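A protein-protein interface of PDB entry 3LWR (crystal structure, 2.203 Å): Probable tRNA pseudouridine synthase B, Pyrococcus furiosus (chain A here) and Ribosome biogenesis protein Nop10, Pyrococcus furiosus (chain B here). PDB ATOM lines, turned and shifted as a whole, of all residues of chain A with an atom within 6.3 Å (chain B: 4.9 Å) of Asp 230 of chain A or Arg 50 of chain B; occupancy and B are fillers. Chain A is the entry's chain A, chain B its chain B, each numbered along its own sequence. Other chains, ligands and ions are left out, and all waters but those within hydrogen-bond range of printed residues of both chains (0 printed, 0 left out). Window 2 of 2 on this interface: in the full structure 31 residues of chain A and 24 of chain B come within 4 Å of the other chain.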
ATOM      1  N   ASP A 222     -22.442   8.689  23.091  1.00  0.00           N
ATOM      2  CA  ASP A 222     -23.770   8.541  22.488  1.00  0.00           C
ATOM      3  C   ASP A 222     -23.873   7.228  21.710  1.00  0.00           C
ATOM      4  O   ASP A 222     -24.868   6.509  21.825  1.00  0.00           O
ATOM      5  CB  ASP A 222     -24.137   9.736  21.608  1.00  0.00           C
ATOM      6  CG  ASP A 222     -24.363  11.010  22.423  1.00  0.00           C
ATOM      7  OD1 ASP A 222     -24.487  10.905  23.656  1.00  0.00           O
ATOM      8  OD2 ASP A 222     -24.411  12.104  21.838  1.00  0.00           O
ATOM      9  N   TYR A 225     -24.278   4.252  24.093  1.00  0.00           N
ATOM     10  CA  TYR A 225     -25.667   4.086  24.512  1.00  0.00           C
ATOM     11  C   TYR A 225     -26.580   3.603  23.386  1.00  0.00           C
ATOM     12  O   TYR A 225     -27.494   2.815  23.621  1.00  0.00           O
ATOM     13  CB  TYR A 225     -26.213   5.375  25.122  1.00  0.00           C
ATOM     14  CG  TYR A 225     -25.649   5.643  26.495  1.00  0.00           C
ATOM     15  CD1 TYR A 225     -24.975   6.823  26.779  1.00  0.00           C
ATOM     16  CD2 TYR A 225     -25.778   4.703  27.504  1.00  0.00           C
ATOM     17  CE1 TYR A 225     -24.446   7.069  28.042  1.00  0.00           C
ATOM     18  CE2 TYR A 225     -25.258   4.935  28.768  1.00  0.00           C
ATOM     19  CZ  TYR A 225     -24.593   6.120  29.030  1.00  0.00           C
ATOM     20  OH  TYR A 225     -24.076   6.338  30.285  1.00  0.00           O
ATOM     21  N   PHE A 226     -26.339   4.079  22.170  1.00  0.00           N
ATOM     22  CA  PHE A 226     -27.088   3.582  21.015  1.00  0.00           C
ATOM     23  C   PHE A 226     -26.898   2.066  20.911  1.00  0.00           C
ATOM     24  O   PHE A 226     -27.801   1.347  20.505  1.00  0.00           O
ATOM     25  CB  PHE A 226     -26.649   4.269  19.716  1.00  0.00           C
ATOM     26  CG  PHE A 226     -26.995   5.716  19.655  1.00  0.00           C
ATOM     27  CD1 PHE A 226     -26.461   6.520  18.671  1.00  0.00           C
ATOM     28  CD2 PHE A 226     -27.844   6.279  20.595  1.00  0.00           C
ATOM     29  CE1 PHE A 226     -26.781   7.866  18.606  1.00  0.00           C
ATOM     30  CE2 PHE A 226     -28.168   7.620  20.541  1.00  0.00           C
ATOM     31  CZ  PHE A 226     -27.635   8.417  19.540  1.00  0.00           C
ATOM     32  N   TRP A 227     -25.720   1.590  21.288  1.00  0.00           N
ATOM     33  CA  TRP A 227     -25.489   0.151  21.379  1.00  0.00           C
ATOM     34  C   TRP A 227     -26.141  -0.510  22.597  1.00  0.00           C
ATOM     35  O   TRP A 227     -26.990  -1.376  22.446  1.00  0.00           O
ATOM     36  CB  TRP A 227     -23.998  -0.156  21.354  1.00  0.00           C
ATOM     37  CG  TRP A 227     -23.697  -1.564  21.682  1.00  0.00           C
ATOM     38  CD1 TRP A 227     -24.322  -2.670  21.188  1.00  0.00           C
ATOM     39  CD2 TRP A 227     -22.676  -2.035  22.560  1.00  0.00           C
ATOM     40  NE1 TRP A 227     -23.752  -3.807  21.713  1.00  0.00           N
ATOM     41  CE2 TRP A 227     -22.746  -3.443  22.564  1.00  0.00           C
ATOM     42  CE3 TRP A 227     -21.715  -1.406  23.355  1.00  0.00           C
ATOM     43  CZ2 TRP A 227     -21.889  -4.232  23.329  1.00  0.00           C
ATOM     44  CZ3 TRP A 227     -20.853  -2.197  24.110  1.00  0.00           C
ATOM     45  CH2 TRP A 227     -20.951  -3.591  24.089  1.00  0.00           C
ATOM     46  N   LYS A 228     -25.747  -0.103  23.798  1.00  0.00           N
ATOM     47  CA  LYS A 228     -26.246  -0.751  25.017  1.00  0.00           C
ATOM     48  C   LYS A 228     -27.758  -0.607  25.233  1.00  0.00           C
ATOM     49  O   LYS A 228     -28.402  -1.538  25.691  1.00  0.00           O
ATOM     50  CB  LYS A 228     -25.515  -0.226  26.259  1.00  0.00           C
ATOM     51  CG  LYS A 228     -24.012  -0.502  26.280  1.00  0.00           C
ATOM     52  CD  LYS A 228     -23.722  -1.996  26.429  1.00  0.00           C
ATOM     53  CE  LYS A 228     -23.842  -2.443  27.886  1.00  0.00           C
ATOM     54  NZ  LYS A 228     -23.410  -3.866  28.079  1.00  0.00           N
ATOM     55  N   GLU A 229     -28.307   0.567  24.926  1.00  0.00           N
ATOM     56  CA  GLU A 229     -29.673   0.896  25.313  1.00  0.00           C
ATOM     57  C   GLU A 229     -30.678   0.819  24.157  1.00  0.00           C
ATOM     58  O   GLU A 229     -31.860   0.561  24.381  1.00  0.00           O
ATOM     59  CB  GLU A 229     -29.728   2.267  26.019  1.00  0.00           C
ATOM     60  CG  GLU A 229     -29.032   2.264  27.408  1.00  0.00           C
ATOM     61  CD  GLU A 229     -29.070   3.620  28.118  1.00  0.00           C
ATOM     62  OE1 GLU A 229     -28.811   3.672  29.353  1.00  0.00           O
ATOM     63  OE2 GLU A 229     -29.357   4.625  27.437  1.00  0.00           O
ATOM     64  N   ASP A 230     -30.209   1.031  22.930  1.00  0.00           N
ATOM     65  CA  ASP A 230     -31.082   0.992  21.763  1.00  0.00           C
ATOM     66  C   ASP A 230     -30.897  -0.300  20.966  1.00  0.00           C
ATOM     67  O   ASP A 230     -31.706  -0.613  20.112  1.00  0.00           O
ATOM     68  CB  ASP A 230     -30.808   2.184  20.831  1.00  0.00           C
ATOM     69  CG  ASP A 230     -31.197   3.529  21.442  1.00  0.00           C
ATOM     70  OD1 ASP A 230     -32.278   4.051  21.095  1.00  0.00           O
ATOM     71  OD2 ASP A 230     -30.420   4.070  22.253  1.00  0.00           O
ATOM     72  N   GLY A 231     -29.815  -1.028  21.217  1.00  0.00           N
ATOM     73  CA  GLY A 231     -29.537  -2.259  20.486  1.00  0.00           C
ATOM     74  C   GLY A 231     -28.911  -2.044  19.111  1.00  0.00           C
ATOM     75  O   GLY A 231     -28.916  -2.954  18.279  1.00  0.00           O
ATOM     76  N   ILE A 232     -28.384  -0.841  18.859  1.00  0.00           N
ATOM     77  CA  ILE A 232     -27.719  -0.554  17.587  1.00  0.00           C
ATOM     78  C   ILE A 232     -26.202  -0.611  17.732  1.00  0.00           C
ATOM     79  O   ILE A 232     -25.591   0.238  18.383  1.00  0.00           O
ATOM     80  CB  ILE A 232     -28.102   0.821  17.020  1.00  0.00           C
ATOM     81  CG1 ILE A 232     -29.617   0.971  16.942  1.00  0.00           C
ATOM     82  CG2 ILE A 232     -27.498   1.001  15.636  1.00  0.00           C
ATOM     83  CD1 ILE A 232     -30.272  -0.145  16.146  1.00  0.00           C
ATOM     84  N   ARG B  46     -29.014  13.101  22.740  1.00  0.00           N
ATOM     85  CA  ARG B  46     -29.178  11.800  22.088  1.00  0.00           C
ATOM     86  C   ARG B  46     -30.473  11.815  21.289  1.00  0.00           C
ATOM     87  O   ARG B  46     -30.534  11.312  20.170  1.00  0.00           O
ATOM     88  CB  ARG B  46     -29.172  10.646  23.113  1.00  0.00           C
ATOM     89  CG  ARG B  46     -27.768  10.092  23.463  1.00  0.00           C
ATOM     90  CD  ARG B  46     -27.730   9.354  24.856  1.00  0.00           C
ATOM     91  NE  ARG B  46     -26.530   9.786  25.564  1.00  0.00           N
ATOM     92  CZ  ARG B  46     -26.462  10.022  26.863  1.00  0.00           C
ATOM     93  NH1 ARG B  46     -27.532   9.850  27.619  1.00  0.00           N
ATOM     94  NH2 ARG B  46     -25.322  10.425  27.410  1.00  0.00           N
ATOM     95  N   ARG B  47     -31.499  12.435  21.858  1.00  0.00           N
ATOM     96  CA  ARG B  47     -32.778  12.553  21.186  1.00  0.00           C
ATOM     97  C   ARG B  47     -32.611  13.276  19.831  1.00  0.00           C
ATOM     98  O   ARG B  47     -33.109  12.803  18.802  1.00  0.00           O
ATOM     99  CB  ARG B  47     -33.772  13.269  22.098  1.00  0.00           C
ATOM    100  CG  ARG B  47     -35.225  13.121  21.694  1.00  0.00           C
ATOM    101  CD  ARG B  47     -36.162  13.360  22.875  1.00  0.00           C
ATOM    102  NE  ARG B  47     -35.963  12.361  23.923  1.00  0.00           N
ATOM    103  CZ  ARG B  47     -36.539  12.407  25.120  1.00  0.00           C
ATOM    104  NH1 ARG B  47     -37.357  13.404  25.426  1.00  0.00           N
ATOM    105  NH2 ARG B  47     -36.294  11.457  26.014  1.00  0.00           N
ATOM    106  N   TRP B  48     -31.884  14.397  19.833  1.00  0.00           N
ATOM    107  CA  TRP B  48     -31.590  15.146  18.604  1.00  0.00           C
ATOM    108  C   TRP B  48     -30.712  14.344  17.646  1.00  0.00           C
ATOM    109  O   TRP B  48     -30.867  14.439  16.432  1.00  0.00           O
ATOM    110  CB  TRP B  48     -30.901  16.472  18.939  1.00  0.00           C
ATOM    111  CG  TRP B  48     -29.973  17.015  17.867  1.00  0.00           C
ATOM    112  CD1 TRP B  48     -30.332  17.597  16.680  1.00  0.00           C
ATOM    113  CD2 TRP B  48     -28.534  17.051  17.909  1.00  0.00           C
ATOM    114  NE1 TRP B  48     -29.205  17.995  15.984  1.00  0.00           N
ATOM    115  CE2 TRP B  48     -28.093  17.668  16.717  1.00  0.00           C
ATOM    116  CE3 TRP B  48     -27.582  16.630  18.844  1.00  0.00           C
ATOM    117  CZ2 TRP B  48     -26.737  17.870  16.432  1.00  0.00           C
ATOM    118  CZ3 TRP B  48     -26.237  16.834  18.566  1.00  0.00           C
ATOM    119  CH2 TRP B  48     -25.826  17.443  17.365  1.00  0.00           C
ATOM    120  N   LYS B  49     -29.796  13.548  18.196  1.00  0.00           N
ATOM    121  CA  LYS B  49     -28.826  12.842  17.369  1.00  0.00           C
ATOM    122  C   LYS B  49     -29.432  11.602  16.695  1.00  0.00           C
ATOM    123  O   LYS B  49     -29.111  11.303  15.542  1.00  0.00           O
ATOM    124  CB  LYS B  49     -27.598  12.483  18.200  1.00  0.00           C
ATOM    125  CG  LYS B  49     -26.484  11.813  17.443  1.00  0.00           C
ATOM    126  CD  LYS B  49     -25.222  11.722  18.309  1.00  0.00           C
ATOM    127  CE  LYS B  49     -24.781  13.112  18.817  1.00  0.00           C
ATOM    128  NZ  LYS B  49     -23.460  13.069  19.555  1.00  0.00           N
ATOM    129  N   ARG B  50     -30.294  10.885  17.411  1.00  0.00           N
ATOM    130  CA  ARG B  50     -31.027   9.756  16.821  1.00  0.00           C
ATOM    131  C   ARG B  50     -31.830  10.213  15.607  1.00  0.00           C
ATOM    132  O   ARG B  50     -31.806   9.571  14.561  1.00  0.00           O
ATOM    133  CB  ARG B  50     -31.965   9.081  17.837  1.00  0.00           C
ATOM    134  CG  ARG B  50     -31.262   8.120  18.774  1.00  0.00           C
ATOM    135  CD  ARG B  50     -32.249   7.288  19.590  1.00  0.00           C
ATOM    136  NE  ARG B  50     -31.631   6.786  20.818  1.00  0.00           N
ATOM    137  CZ  ARG B  50     -31.605   7.457  21.969  1.00  0.00           C
ATOM    138  NH1 ARG B  50     -32.169   8.657  22.058  1.00  0.00           N
ATOM    139  NH2 ARG B  50     -31.021   6.929  23.035  1.00  0.00           N
ATOM    140  N   GLU B  51     -32.533  11.329  15.757  1.00  0.00           N
ATOM    141  CA  GLU B  51     -33.285  11.917  14.661  1.00  0.00           C
ATOM    142  C   GLU B  51     -32.373  12.252  13.477  1.00  0.00           C
ATOM    143  O   GLU B  51     -32.662  11.869  12.345  1.00  0.00           O
ATOM    144  CB  GLU B  51     -34.049  13.159  15.128  1.00  0.00           C
ATOM    145  CG  GLU B  51     -35.069  13.667  14.115  1.00  0.00           C
ATOM    146  CD  GLU B  51     -36.152  14.539  14.743  1.00  0.00           C
ATOM    147  OE1 GLU B  51     -36.327  14.479  15.981  1.00  0.00           O
ATOM    148  OE2 GLU B  51     -36.833  15.280  13.999  1.00  0.00           O
ATOM    149  N   VAL B  52     -31.272  12.955  13.736  1.00  0.00           N
ATOM    150  CA  VAL B  52     -30.294  13.251  12.679  1.00  0.00           C
ATOM    151  C   VAL B  52     -29.821  11.978  11.956  1.00  0.00           C
ATOM    152  O   VAL B  52     -29.688  11.969  10.735  1.00  0.00           O
ATOM    153  CB  VAL B  52     -29.060  14.039  13.214  1.00  0.00           C
ATOM    154  CG1 VAL B  52     -27.876  13.909  12.261  1.00  0.00           C
ATOM    155  CG2 VAL B  52     -29.399  15.520  13.446  1.00  0.00           C
ATOM    156  N   LEU B  53     -29.581  10.904  12.706  1.00  0.00           N
ATOM    157  CA  LEU B  53     -29.066   9.662  12.122  1.00  0.00           C
ATOM    158  C   LEU B  53     -30.164   8.686  11.646  1.00  0.00           C
ATOM    159  O   LEU B  53     -29.865   7.637  11.077  1.00  0.00           O
ATOM    160  CB  LEU B  53     -28.149   8.947  13.117  1.00  0.00           C
ATOM    161  CG  LEU B  53     -26.895   9.688  13.580  1.00  0.00           C
ATOM    162  CD1 LEU B  53     -26.376   9.058  14.859  1.00  0.00           C
ATOM    163  CD2 LEU B  53     -25.820   9.661  12.495  1.00  0.00           C
ATOM    164  N   GLY B  54     -31.425   9.019  11.888  1.00  0.00           N
ATOM    165  CA  GLY B  54     -32.522   8.139  11.506  1.00  0.00           C
ATOM    166  C   GLY B  54     -32.550   6.811  12.248  1.00  0.00           C
ATOM    167  O   GLY B  54     -32.901   5.769  11.689  1.00  0.00           O
ATOM    168  N   ILE B  55     -32.173   6.851  13.520  1.00  0.00           N
ATOM    169  CA  ILE B  55     -32.186   5.664  14.360  1.00  0.00           C
ATOM    170  C   ILE B  55     -33.588   5.401  14.881  1.00  0.00           C
ATOM    171  O   ILE B  55     -34.373   6.335  15.031  1.00  0.00           O
ATOM    172  CB  ILE B  55     -31.221   5.826  15.544  1.00  0.00           C
ATOM    173  CG1 ILE B  55     -29.788   5.582  15.076  1.00  0.00           C
ATOM    174  CG2 ILE B  55     -31.589   4.871  16.675  1.00  0.00           C
ATOM    175  CD1 ILE B  55     -28.760   5.696  16.173  1.00  0.00           C
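The backbone carbonyl oxygen (O) of Tyr 225 of chain A sits at hydrogen-bond distance from the backbone NH (N) of Asp 230 of chain A (3.3 Å).
The backbone carbonyl oxygen (O) of Phe 226 of chain A is in hydrogen-bond range of the backbone NH (N) of Gly 231 of chain A, 3.2 Å away.
O of Phe 226 of chain A lies within hydrogen-bond range of N of Ile 232 of chain A (2.8 Å).
The backbone carbonyl oxygen (O) of Arg 50 of chain B is in hydrogen-bond range of the backbone NH (N) of Ile 55 of chain B (2.9 Å).
Printed residues of chain B within 4 Å of Phe 226 of chain A: Arg 46, Arg 50, Leu 53 and Ile 55.
Of chain B, only Arg 50 (2.8 Å) comes within 4 Å of Asp 230 of chain A.
Printed residues of chain A within 4 Å of Arg 46 of chain B: Asp 222 (3.0 Å), Tyr 225 (3.5 Å) and Phe 226 (3.8 Å).
Of chain A, only Phe 226 and Asp 230 come within 4 Å of Arg 50 of chain B.
Glu 51 of chain B touches none of the printed residues of chain A.
Of the printed residues of chain A, Leu 53 of chain B touches Phe 226 (3.95 Å).
The nearest residue of chain B that does not touch Asp 230 of chain A is Ile 55 of chain B (4.5 Å).
The nearest residue of chain A that does not touch Arg 50 of chain B is Glu 229 of chain A (5.2 Å).
The side-chain carboxylate (OD1) of Asp 222 of chain A lies within salt-bridge range of the guanidinium group (NE) of Arg 46 of chain B.
The side-chain carboxylate (OD2) of Asp 222 of chain A lies within salt-bridge range of the side-chain amino group (NZ) of Lys 49 of chain B (2.7 Å).
The guanidinium group (NE) of Arg 50 of chain B lies within salt-bridge range of the side-chain carboxylate (OD1) of Asp 230 of chain A (2.8 Å).
Among the printed residues, pairs that only touch across the chains: Tyr 225 of chain A with Arg 46 of chain B (3.5 Å), Phe 226 of chain A with Arg 46 of chain B (3.8 Å), Phe 226 of chain A with Arg 50 of chain B (3.6 Å), Phe 226 of chain A with Leu 53 of chain B (3.95 Å) and Phe 226 of chain A with Ile 55 of chain B (3.5 Å).
Of the 10 printed residues of chain B, 5 touch a printed residue of chain A.
Along chain B the printed residues that touch a printed residue of chain A span positions 46 to 55.
Of the 9 printed residues of chain A, 4 touch a printed residue of chain B.
Hydrophobic or aromatic side chains of chain A within 4 Å of the printed part of chain B: Tyr 225 and Phe 226.
Among the printed residues, 8 pairs touch across the chains.
Among the printed residues, Asp or Glu carboxylates within 4 Å of a Lys or Arg side-chain nitrogen of the other chain: Asp 222 of chain A with Arg 46 of chain B, Asp 222 of chain A with Lys 49 of chain B and Asp 230 of chain A with Arg 50 of chain B.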
